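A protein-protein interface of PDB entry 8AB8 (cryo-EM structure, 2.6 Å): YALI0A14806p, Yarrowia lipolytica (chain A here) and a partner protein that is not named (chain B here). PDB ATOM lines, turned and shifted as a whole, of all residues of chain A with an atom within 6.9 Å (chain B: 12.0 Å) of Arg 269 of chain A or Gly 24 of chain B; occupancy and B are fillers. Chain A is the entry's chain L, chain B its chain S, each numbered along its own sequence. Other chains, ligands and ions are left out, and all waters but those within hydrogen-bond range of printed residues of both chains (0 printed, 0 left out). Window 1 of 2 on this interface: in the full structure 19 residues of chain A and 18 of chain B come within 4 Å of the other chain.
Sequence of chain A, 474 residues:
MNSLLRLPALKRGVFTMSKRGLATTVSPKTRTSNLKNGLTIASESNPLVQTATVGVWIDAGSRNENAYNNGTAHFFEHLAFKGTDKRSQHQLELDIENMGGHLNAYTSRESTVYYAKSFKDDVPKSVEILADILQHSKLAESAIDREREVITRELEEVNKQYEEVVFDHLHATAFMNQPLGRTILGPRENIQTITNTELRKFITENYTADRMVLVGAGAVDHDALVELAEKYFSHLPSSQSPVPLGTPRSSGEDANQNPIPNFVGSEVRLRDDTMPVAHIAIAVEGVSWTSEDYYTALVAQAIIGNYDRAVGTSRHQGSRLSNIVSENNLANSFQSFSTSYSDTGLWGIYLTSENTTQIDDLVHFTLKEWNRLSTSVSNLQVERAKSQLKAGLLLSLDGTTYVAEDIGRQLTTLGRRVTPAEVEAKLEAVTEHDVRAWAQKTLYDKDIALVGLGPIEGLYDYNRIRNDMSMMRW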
ATOM      1  N   GLU A 267       2.535  26.075  21.019  1.00  0.00           N
ATOM      2  CA  GLU A 267       3.279  26.057  19.776  1.00  0.00           C
ATOM      3  C   GLU A 267       3.168  27.410  19.105  1.00  0.00           C
ATOM      4  O   GLU A 267       2.170  28.111  19.257  1.00  0.00           O
ATOM      5  CB  GLU A 267       2.865  24.923  18.843  1.00  0.00           C
ATOM      6  CG  GLU A 267       1.382  24.754  18.803  1.00  0.00           C
ATOM      7  CD  GLU A 267       0.908  23.892  17.652  1.00  0.00           C
ATOM      8  OE1 GLU A 267       1.431  22.761  17.490  1.00  0.00           O
ATOM      9  OE2 GLU A 267      -0.002  24.341  16.925  1.00  0.00           O
ATOM     10  N   VAL A 268       4.241  27.757  18.402  1.00  0.00           N
ATOM     11  CA  VAL A 268       4.259  28.871  17.483  1.00  0.00           C
ATOM     12  C   VAL A 268       4.598  28.289  16.123  1.00  0.00           C
ATOM     13  O   VAL A 268       5.619  27.617  15.986  1.00  0.00           O
ATOM     14  CB  VAL A 268       5.320  29.906  17.891  1.00  0.00           C
ATOM     15  CG1 VAL A 268       5.307  31.094  16.946  1.00  0.00           C
ATOM     16  CG2 VAL A 268       5.145  30.366  19.331  1.00  0.00           C
ATOM     17  N   ARG A 269       3.751  28.567  15.129  1.00  0.00           N
ATOM     18  CA  ARG A 269       4.071  28.175  13.766  1.00  0.00           C
ATOM     19  C   ARG A 269       4.306  29.427  12.937  1.00  0.00           C
ATOM     20  O   ARG A 269       3.441  30.296  12.882  1.00  0.00           O
ATOM     21  CB  ARG A 269       2.947  27.344  13.151  1.00  0.00           C
ATOM     22  CG  ARG A 269       2.611  26.103  13.961  1.00  0.00           C
ATOM     23  CD  ARG A 269       1.292  25.482  13.585  1.00  0.00           C
ATOM     24  NE  ARG A 269       1.745  24.265  12.953  1.00  0.00           N
ATOM     25  CZ  ARG A 269       1.844  23.072  13.523  1.00  0.00           C
ATOM     26  NH1 ARG A 269       1.420  22.826  14.753  1.00  0.00           N
ATOM     27  NH2 ARG A 269       2.338  22.100  12.791  1.00  0.00           N
ATOM     28  N   LEU A 270       5.470  29.499  12.286  1.00  0.00           N
ATOM     29  CA  LEU A 270       5.825  30.633  11.458  1.00  0.00           C
ATOM     30  C   LEU A 270       6.069  30.082  10.068  1.00  0.00           C
ATOM     31  O   LEU A 270       7.202  29.943   9.631  1.00  0.00           O
ATOM     32  CB  LEU A 270       7.072  31.311  12.030  1.00  0.00           C
ATOM     33  CG  LEU A 270       6.960  31.722  13.496  1.00  0.00           C
ATOM     34  CD1 LEU A 270       8.326  31.904  14.143  1.00  0.00           C
ATOM     35  CD2 LEU A 270       6.120  32.977  13.654  1.00  0.00           C
ATOM     36  N   ARG A 271       4.983  29.675   9.424  1.00  0.00           N
ATOM     37  CA  ARG A 271       5.132  29.013   8.148  1.00  0.00           C
ATOM     38  C   ARG A 271       5.588  30.030   7.113  1.00  0.00           C
ATOM     39  O   ARG A 271       5.078  31.145   7.069  1.00  0.00           O
ATOM     40  CB  ARG A 271       3.810  28.382   7.739  1.00  0.00           C
ATOM     41  CG  ARG A 271       3.809  27.863   6.312  1.00  0.00           C
ATOM     42  CD  ARG A 271       2.769  26.785   6.256  1.00  0.00           C
ATOM     43  NE  ARG A 271       2.571  26.457   4.861  1.00  0.00           N
ATOM     44  CZ  ARG A 271       1.553  25.737   4.415  1.00  0.00           C
ATOM     45  NH1 ARG A 271       0.641  25.288   5.262  1.00  0.00           N
ATOM     46  NH2 ARG A 271       1.448  25.478   3.126  1.00  0.00           N
ATOM     47  N   LEU A 450       6.767  24.052  21.168  1.00  0.00           N
ATOM     48  CA  LEU A 450       7.140  23.661  19.827  1.00  0.00           C
ATOM     49  C   LEU A 450       7.165  24.914  18.966  1.00  0.00           C
ATOM     50  O   LEU A 450       6.232  25.699  19.012  1.00  0.00           O
ATOM     51  CB  LEU A 450       6.076  22.660  19.375  1.00  0.00           C
ATOM     52  CG  LEU A 450       5.962  22.405  17.878  1.00  0.00           C
ATOM     53  CD1 LEU A 450       7.117  21.548  17.395  1.00  0.00           C
ATOM     54  CD2 LEU A 450       4.646  21.695  17.594  1.00  0.00           C
ATOM     55  N   VAL A 451       8.252  25.120  18.225  1.00  0.00           N
ATOM     56  CA  VAL A 451       8.315  26.241  17.304  1.00  0.00           C
ATOM     57  C   VAL A 451       8.733  25.696  15.954  1.00  0.00           C
ATOM     58  O   VAL A 451       9.700  24.952  15.874  1.00  0.00           O
ATOM     59  CB  VAL A 451       9.291  27.335  17.770  1.00  0.00           C
ATOM     60  CG1 VAL A 451       9.444  28.430  16.724  1.00  0.00           C
ATOM     61  CG2 VAL A 451       8.874  27.929  19.106  1.00  0.00           C
ATOM     62  N   GLY A 452       7.995  26.069  14.912  1.00  0.00           N
ATOM     63  CA  GLY A 452       8.334  25.667  13.562  1.00  0.00           C
ATOM     64  C   GLY A 452       8.431  26.899  12.675  1.00  0.00           C
ATOM     65  O   GLY A 452       7.581  27.781  12.743  1.00  0.00           O
ATOM     66  N   LEU A 453       9.491  26.973  11.873  1.00  0.00           N
ATOM     67  CA  LEU A 453       9.680  28.122  11.011  1.00  0.00           C
ATOM     68  C   LEU A 453      10.066  27.622   9.623  1.00  0.00           C
ATOM     69  O   LEU A 453      10.898  26.728   9.492  1.00  0.00           O
ATOM     70  CB  LEU A 453      10.747  29.018  11.652  1.00  0.00           C
ATOM     71  CG  LEU A 453      11.441  30.020  10.727  1.00  0.00           C
ATOM     72  CD1 LEU A 453      10.537  31.195  10.412  1.00  0.00           C
ATOM     73  CD2 LEU A 453      12.725  30.527  11.363  1.00  0.00           C
ATOM     74  N   GLY A 454       9.422  28.169   8.590  1.00  0.00           N
ATOM     75  CA  GLY A 454       9.755  27.785   7.233  1.00  0.00           C
ATOM     76  C   GLY A 454       8.689  26.898   6.597  1.00  0.00           C
ATOM     77  O   GLY A 454       7.495  27.067   6.833  1.00  0.00           O
ATOM     78  N   ILE A 456       6.708  24.251   6.793  1.00  0.00           N
ATOM     79  CA  ILE A 456       6.412  23.331   7.878  1.00  0.00           C
ATOM     80  C   ILE A 456       4.990  22.813   7.725  1.00  0.00           C
ATOM     81  O   ILE A 456       4.397  22.366   8.704  1.00  0.00           O
ATOM     82  CB  ILE A 456       6.589  24.038   9.235  1.00  0.00           C
ATOM     83  CG1 ILE A 456       5.775  25.340   9.272  1.00  0.00           C
ATOM     84  CG2 ILE A 456       8.064  24.260   9.525  1.00  0.00           C
ATOM     85  CD1 ILE A 456       5.481  25.908  10.646  1.00  0.00           C
ATOM     86  N   GLU A 457       4.447  22.895   6.505  1.00  0.00           N
ATOM     87  CA  GLU A 457       3.129  22.355   6.205  1.00  0.00           C
ATOM     88  C   GLU A 457       3.009  20.931   6.745  1.00  0.00           C
ATOM     89  O   GLU A 457       1.971  20.570   7.290  1.00  0.00           O
ATOM     90  CB  GLU A 457       2.847  22.350   4.705  1.00  0.00           C
ATOM     91  CG  GLU A 457       1.467  21.812   4.373  1.00  0.00           C
ATOM     92  CD  GLU A 457       1.173  21.705   2.891  1.00  0.00           C
ATOM     93  OE1 GLU A 457       0.804  22.731   2.276  1.00  0.00           O
ATOM     94  OE2 GLU A 457       1.311  20.592   2.356  1.00  0.00           O
ATOM     95  N   GLY A 458       4.075  20.136   6.592  1.00  0.00           N
ATOM     96  CA  GLY A 458       4.066  18.741   6.993  1.00  0.00           C
ATOM     97  C   GLY A 458       4.300  18.537   8.489  1.00  0.00           C
ATOM     98  O   GLY A 458       4.364  17.401   8.957  1.00  0.00           O
ATOM     99  N   LEU A 459       4.467  19.615   9.250  1.00  0.00           N
ATOM    100  CA  LEU A 459       4.542  19.425  10.686  1.00  0.00           C
ATOM    101  C   LEU A 459       3.106  19.255  11.172  1.00  0.00           C
ATOM    102  O   LEU A 459       2.300  20.134  10.908  1.00  0.00           O
ATOM    103  CB  LEU A 459       5.214  20.662  11.277  1.00  0.00           C
ATOM    104  CG  LEU A 459       5.345  20.674  12.797  1.00  0.00           C
ATOM    105  CD1 LEU A 459       6.238  19.539  13.269  1.00  0.00           C
ATOM    106  CD2 LEU A 459       5.867  22.014  13.296  1.00  0.00           C
ATOM    107  N   TYR A 460       2.757  18.122  11.804  1.00  0.00           N
ATOM    108  CA  TYR A 460       1.367  17.925  12.197  1.00  0.00           C
ATOM    109  C   TYR A 460       1.001  18.857  13.342  1.00  0.00           C
ATOM    110  O   TYR A 460       1.870  19.508  13.910  1.00  0.00           O
ATOM    111  CB  TYR A 460       1.095  16.488  12.635  1.00  0.00           C
ATOM    112  CG  TYR A 460       1.179  15.486  11.516  1.00  0.00           C
ATOM    113  CD1 TYR A 460       0.657  15.766  10.260  1.00  0.00           C
ATOM    114  CD2 TYR A 460       1.777  14.250  11.716  1.00  0.00           C
ATOM    115  CE1 TYR A 460       0.735  14.845   9.226  1.00  0.00           C
ATOM    116  CE2 TYR A 460       1.860  13.315  10.692  1.00  0.00           C
ATOM    117  CZ  TYR A 460       1.337  13.616   9.445  1.00  0.00           C
ATOM    118  OH  TYR A 460       1.404  12.712   8.426  1.00  0.00           O
ATOM    119  N   ASP A 461      -0.282  18.893  13.686  1.00  0.00           N
ATOM    120  CA  ASP A 461      -0.807  19.747  14.736  1.00  0.00           C
ATOM    121  C   ASP A 461      -0.247  19.335  16.102  1.00  0.00           C
ATOM    122  O   ASP A 461       0.345  18.262  16.250  1.00  0.00           O
ATOM    123  CB  ASP A 461      -2.332  19.657  14.694  1.00  0.00           C
ATOM    124  CG  ASP A 461      -2.785  18.216  14.522  1.00  0.00           C
ATOM    125  OD1 ASP A 461      -2.577  17.444  15.472  1.00  0.00           O
ATOM    126  OD2 ASP A 461      -3.310  17.866  13.424  1.00  0.00           O
ATOM    127  N   TYR A 462      -0.479  20.189  17.107  1.00  0.00           N
ATOM    128  CA  TYR A 462       0.029  19.977  18.452  1.00  0.00           C
ATOM    129  C   TYR A 462      -0.252  18.567  18.976  1.00  0.00           C
ATOM    130  O   TYR A 462       0.675  17.937  19.470  1.00  0.00           O
ATOM    131  CB  TYR A 462      -0.426  21.070  19.422  1.00  0.00           C
ATOM    132  CG  TYR A 462       0.312  21.027  20.735  1.00  0.00           C
ATOM    133  CD1 TYR A 462      -0.147  20.232  21.782  1.00  0.00           C
ATOM    134  CD2 TYR A 462       1.482  21.751  20.934  1.00  0.00           C
ATOM    135  CE1 TYR A 462       0.534  20.153  22.988  1.00  0.00           C
ATOM    136  CE2 TYR A 462       2.176  21.685  22.139  1.00  0.00           C
ATOM    137  CZ  TYR A 462       1.701  20.883  23.170  1.00  0.00           C
ATOM    138  OH  TYR A 462       2.373  20.806  24.366  1.00  0.00           O
ATOM    139  N   ILE A 465       1.858  15.723  17.584  1.00  0.00           N
ATOM    140  CA  ILE A 465       3.225  15.811  18.076  1.00  0.00           C
ATOM    141  C   ILE A 465       3.258  15.340  19.526  1.00  0.00           C
ATOM    142  O   ILE A 465       4.039  14.463  19.871  1.00  0.00           O
ATOM    143  CB  ILE A 465       3.867  17.211  17.925  1.00  0.00           C
ATOM    144  CG1 ILE A 465       3.764  17.828  16.523  1.00  0.00           C
ATOM    145  CG2 ILE A 465       5.301  17.187  18.432  1.00  0.00           C
ATOM    146  CD1 ILE A 465       3.982  16.878  15.368  1.00  0.00           C
ATOM    147  N   TRP B  11       0.482  15.997   2.720  1.00  0.00           N
ATOM    148  CA  TRP B  11       1.284  16.766   3.656  1.00  0.00           C
ATOM    149  C   TRP B  11       2.627  17.158   3.046  1.00  0.00           C
ATOM    150  O   TRP B  11       3.339  16.311   2.519  1.00  0.00           O
ATOM    151  CB  TRP B  11       1.494  15.961   4.928  1.00  0.00           C
ATOM    152  CG  TRP B  11       0.204  15.600   5.586  1.00  0.00           C
ATOM    153  CD1 TRP B  11      -0.393  14.375   5.597  1.00  0.00           C
ATOM    154  CD2 TRP B  11      -0.660  16.486   6.319  1.00  0.00           C
ATOM    155  NE1 TRP B  11      -1.561  14.434   6.304  1.00  0.00           N
ATOM    156  CE2 TRP B  11      -1.754  15.713   6.759  1.00  0.00           C
ATOM    157  CE3 TRP B  11      -0.614  17.849   6.649  1.00  0.00           C
ATOM    158  CZ2 TRP B  11      -2.796  16.261   7.511  1.00  0.00           C
ATOM    159  CZ3 TRP B  11      -1.638  18.389   7.398  1.00  0.00           C
ATOM    160  CH2 TRP B  11      -2.720  17.605   7.814  1.00  0.00           C
ATOM    161  N   GLY B  12       2.968  18.445   3.144  1.00  0.00           N
ATOM    162  CA  GLY B  12       4.187  18.953   2.547  1.00  0.00           C
ATOM    163  C   GLY B  12       3.933  19.603   1.189  1.00  0.00           C
ATOM    164  O   GLY B  12       4.672  20.506   0.795  1.00  0.00           O
ATOM    165  N   MET B  14       0.366  20.315  -0.153  1.00  0.00           N
ATOM    166  CA  MET B  14      -1.081  20.183  -0.141  1.00  0.00           C
ATOM    167  C   MET B  14      -1.716  20.872  -1.350  1.00  0.00           C
ATOM    168  O   MET B  14      -2.778  20.453  -1.794  1.00  0.00           O
ATOM    169  CB  MET B  14      -1.692  20.743   1.146  1.00  0.00           C
ATOM    170  CG  MET B  14      -3.079  20.192   1.449  1.00  0.00           C
ATOM    171  SD  MET B  14      -3.084  18.417   1.852  1.00  0.00           S
ATOM    172  CE  MET B  14      -2.090  18.420   3.345  1.00  0.00           C
ATOM    173  N   GLN B  19       2.348  30.315   1.573  1.00  0.00           N
ATOM    174  CA  GLN B  19       1.921  31.036   2.757  1.00  0.00           C
ATOM    175  C   GLN B  19       3.132  31.751   3.328  1.00  0.00           C
ATOM    176  O   GLN B  19       4.220  31.176   3.389  1.00  0.00           O
ATOM    177  CB  GLN B  19       1.333  30.076   3.785  1.00  0.00           C
ATOM    178  CG  GLN B  19       0.260  29.170   3.214  1.00  0.00           C
ATOM    179  CD  GLN B  19      -0.549  28.483   4.289  1.00  0.00           C
ATOM    180  OE1 GLN B  19      -0.294  28.625   5.486  1.00  0.00           O
ATOM    181  NE2 GLN B  19      -1.555  27.735   3.863  1.00  0.00           N
ATOM    182  N   LYS B  20       2.933  33.014   3.695  1.00  0.00           N
ATOM    183  CA  LYS B  20       3.970  33.784   4.348  1.00  0.00           C
ATOM    184  C   LYS B  20       3.308  34.883   5.170  1.00  0.00           C
ATOM    185  O   LYS B  20       2.295  35.439   4.755  1.00  0.00           O
ATOM    186  CB  LYS B  20       4.911  34.378   3.301  1.00  0.00           C
ATOM    187  CG  LYS B  20       6.169  35.005   3.869  1.00  0.00           C
ATOM    188  CD  LYS B  20       7.176  35.332   2.802  1.00  0.00           C
ATOM    189  CE  LYS B  20       8.343  36.125   3.349  1.00  0.00           C
ATOM    190  NZ  LYS B  20       9.206  36.641   2.259  1.00  0.00           N
ATOM    191  N   GLY B  21       3.886  35.176   6.338  1.00  0.00           N
ATOM    192  CA  GLY B  21       3.460  36.320   7.119  1.00  0.00           C
ATOM    193  C   GLY B  21       2.436  35.988   8.200  1.00  0.00           C
ATOM    194  O   GLY B  21       2.081  36.873   8.977  1.00  0.00           O
ATOM    195  N   ILE B  22       1.983  34.730   8.279  1.00  0.00           N
ATOM    196  CA  ILE B  22       1.024  34.364   9.309  1.00  0.00           C
ATOM    197  C   ILE B  22       1.747  33.624  10.428  1.00  0.00           C
ATOM    198  O   ILE B  22       2.387  32.612  10.172  1.00  0.00           O
ATOM    199  CB  ILE B  22      -0.093  33.485   8.721  1.00  0.00           C
ATOM    200  CG1 ILE B  22      -0.759  34.116   7.499  1.00  0.00           C
ATOM    201  CG2 ILE B  22      -1.102  33.096   9.796  1.00  0.00           C
ATOM    202  CD1 ILE B  22      -1.485  33.116   6.616  1.00  0.00           C
ATOM    203  N   ALA B  23       1.612  34.092  11.666  1.00  0.00           N
ATOM    204  CA  ALA B  23       2.098  33.325  12.800  1.00  0.00           C
ATOM    205  C   ALA B  23       0.889  32.732  13.513  1.00  0.00           C
ATOM    206  O   ALA B  23      -0.067  33.455  13.778  1.00  0.00           O
ATOM    207  CB  ALA B  23       2.878  34.233  13.711  1.00  0.00           C
ATOM    208  N   GLY B  24       0.918  31.427  13.799  1.00  0.00           N
ATOM    209  CA  GLY B  24      -0.180  30.773  14.495  1.00  0.00           C
ATOM    210  C   GLY B  24       0.243  30.349  15.896  1.00  0.00           C
ATOM    211  O   GLY B  24       1.377  29.931  16.090  1.00  0.00           O
ATOM    212  N   TYR B  25      -0.659  30.479  16.865  1.00  0.00           N
ATOM    213  CA  TYR B  25      -0.325  30.169  18.243  1.00  0.00           C
ATOM    214  C   TYR B  25      -1.427  29.315  18.838  1.00  0.00           C
ATOM    215  O   TYR B  25      -2.603  29.554  18.568  1.00  0.00           O
ATOM    216  CB  TYR B  25      -0.273  31.455  19.066  1.00  0.00           C
ATOM    217  CG  TYR B  25       0.720  32.461  18.555  1.00  0.00           C
ATOM    218  CD1 TYR B  25       0.412  33.279  17.476  1.00  0.00           C
ATOM    219  CD2 TYR B  25       1.975  32.577  19.137  1.00  0.00           C
ATOM    220  CE1 TYR B  25       1.326  34.204  16.993  1.00  0.00           C
ATOM    221  CE2 TYR B  25       2.901  33.490  18.662  1.00  0.00           C
ATOM    222  CZ  TYR B  25       2.569  34.307  17.594  1.00  0.00           C
ATOM    223  OH  TYR B  25       3.472  35.207  17.127  1.00  0.00           O
ATOM    224  N   THR B  26      -1.052  28.342  19.668  1.00  0.00           N
ATOM    225  CA  THR B  26      -2.062  27.651  20.444  1.00  0.00           C
ATOM    226  C   THR B  26      -1.427  27.021  21.669  1.00  0.00           C
ATOM    227  O   THR B  26      -0.209  26.932  21.759  1.00  0.00           O
ATOM    228  CB  THR B  26      -2.832  26.620  19.611  1.00  0.00           C
ATOM    229  OG1 THR B  26      -3.988  26.323  20.394  1.00  0.00           O
ATOM    230  CG2 THR B  26      -2.050  25.353  19.338  1.00  0.00           C
ATOM    231  N   ILE B  27      -2.268  26.537  22.580  1.00  0.00           N
ATOM    232  CA  ILE B  27      -1.760  25.934  23.794  1.00  0.00           C
ATOM    233  C   ILE B  27      -2.210  24.479  23.864  1.00  0.00           C
ATOM    234  O   ILE B  27      -3.193  24.089  23.238  1.00  0.00           O
ATOM    235  CB  ILE B  27      -2.209  26.746  25.021  1.00  0.00           C
ATOM    236  CG1 ILE B  27      -3.734  26.777  25.128  1.00  0.00           C
ATOM    237  CG2 ILE B  27      -1.603  28.148  24.994  1.00  0.00           C
ATOM    238  CD1 ILE B  27      -4.258  27.277  26.464  1.00  0.00           C
ATOM    239  N   SER B  28      -1.496  23.708  24.685  1.00  0.00           N
ATOM    240  CA  SER B  28      -1.699  22.288  24.898  1.00  0.00           C
ATOM    241  C   SER B  28      -3.118  21.994  25.391  1.00  0.00           C
ATOM    242  O   SER B  28      -3.682  22.779  26.142  1.00  0.00           O
ATOM    243  CB  SER B  28      -0.682  21.830  25.898  1.00  0.00           C
ATOM    244  OG  SER B  28      -0.937  20.504  26.321  1.00  0.00           O
ATOM    245  N   PRO B  29      -3.737  20.845  25.027  1.00  0.00           N
ATOM    246  CA  PRO B  29      -5.017  20.449  25.615  1.00  0.00           C
ATOM    247  C   PRO B  29      -4.943  20.328  27.133  1.00  0.00           C
ATOM    248  O   PRO B  29      -5.924  20.615  27.809  1.00  0.00           O
ATOM    249  CB  PRO B  29      -5.318  19.079  24.986  1.00  0.00           C
ATOM    250  CG  PRO B  29      -3.978  18.592  24.509  1.00  0.00           C
ATOM    251  CD  PRO B  29      -3.251  19.843  24.065  1.00  0.00           C
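Glu 267 of chain A touches Gly 24 of chain B (O to O, 3.7 Å).
Glu 267 of chain A touches Tyr 25 of chain B (O to CA, 3.4 Å).
Val 268 of chain A touches Tyr 25 of chain B (CG1 to CE2, 3.8 Å).
Arg 269 of chain A touches Ala 23 of chain B.
Leu 270 of chain A touches Ala 23 of chain B (CD2 to CB, 3.5 Å).
Ile 22 of chain B touches Arg 271 of chain A (O to N, 3.99 Å).
N of Gly 12 of chain B touches N of Gly 458 of chain A (3.997 Å).
CE2 of Trp 11 of chain B touches CE1 of Tyr 460 of chain A (3.6 Å).
OH of Tyr 462 of chain A touches CB of Ser 28 of chain B, at 3.6 Å.
Pro 29 of chain B touches Tyr 462 of chain A (CD to CD1, 3.9 Å).
OE1 of Gln 19 of chain B lies within hydrogen-bond range of NH1 of Arg 271 of chain A.
The backbone NH (N) of Glu 267 of chain A lies within hydrogen-bond range of the backbone carbonyl oxygen (O) of Thr 26 of chain B (3.0 Å).
The side-chain carboxylate (OE2) of Glu 457 of chain A sits at hydrogen-bond distance from the backbone NH (N) of Gly 12 of chain B (2.8 Å).
OE2 of Glu 457 of chain A sits at hydrogen-bond distance from N of Met 14 of chain B (2.7 Å).
The backbone NH (N) of Arg 269 of chain A lies within hydrogen-bond range of the backbone carbonyl oxygen (O) of Gly 24 of chain B.
Of chain B, only Ile 22 (3.7 Å), Ala 23 (3.3 Å) and Gly 24 (2.9 Å) come within 4 Å of Arg 269 of chain A.
Of the printed residues of chain A, Gly 24 of chain B touches Glu 267 (3.7 Å), Val 268 (3.4 Å) and Arg 269 (2.9 Å).
Val 268 of chain A touches just these residues of chain B: Gly 24 and Tyr 25.
Of chain B, only Ala 23 (3.5 Å) comes within 4 Å of Leu 270 of chain A.
No residue of chain B comes within 4 Å of Gly 452 of chain A.
No residue of chain B comes within 4 Å of Ile 456 of chain A.
No residue of chain B comes within 4 Å of Leu 459 of chain A.
No residue of chain B comes within 4 Å of Asp 461 of chain A.
Of the printed residues of chain B, Arg 271 of chain A touches Gln 19 (3.5 Å), Lys 20 (3.9 Å) and Ile 22 (3.99 Å).
Of the printed residues of chain A, Thr 26 of chain B touches Glu 267 (3.0 Å).
Of the printed residues of chain B, Tyr 460 of chain A touches Trp 11 (3.6 Å).
Leu 453 of chain A touches none of the printed residues of chain B.
The nearest residue of chain B that does not touch Arg 269 of chain A is Tyr 25 of chain B (5.1 Å).
The nearest residue of chain A that does not touch Gly 24 of chain B is Leu 270 of chain A (5.2 Å).
The nearest printed residue of chain B that does not touch Glu 457 of chain A is Gln 19 of chain B (5.8 Å).
The backbone carbonyl oxygen (O) of Val 268 of chain A is in hydrogen-bond range of the backbone NH (N) of Gly 452 of chain A (3.0 Å).
The side-chain carboxylate (OE1) of Glu 267 of chain A lies close to the backbone NH (N) of Tyr 462 of chain A, at 3.2 Å.
O of Tyr 460 of chain A lies within hydrogen-bond range of NH2 of Arg 269 of chain A (2.9 Å).
O of Gly 452 of chain A lies within hydrogen-bond range of N of Leu 270 of chain A (2.8 Å).
The side-chain carboxylate (OE1) of Glu 457 of chain A is in salt-bridge range of the guanidinium group (NH2) of Arg 271 of chain A (2.9 Å).
The backbone carbonyl oxygen (O) of Leu 270 of chain A lies within hydrogen-bond range of the backbone NH (N) of Gly 454 of chain A (3.0 Å).
Hydrophobic or aromatic side chains of chain A that line the printed part of chain B: Val 268, Leu 270, Tyr 460 and Tyr 462.
Of the 14 printed residues of chain B, 12 touch a printed residue of chain A.
Among the printed residues, 19 pairs touch across the chains.
Among the printed residues, no Asp or Glu carboxylate lies within 4 Å of a Lys or Arg side-chain nitrogen of the other chain.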
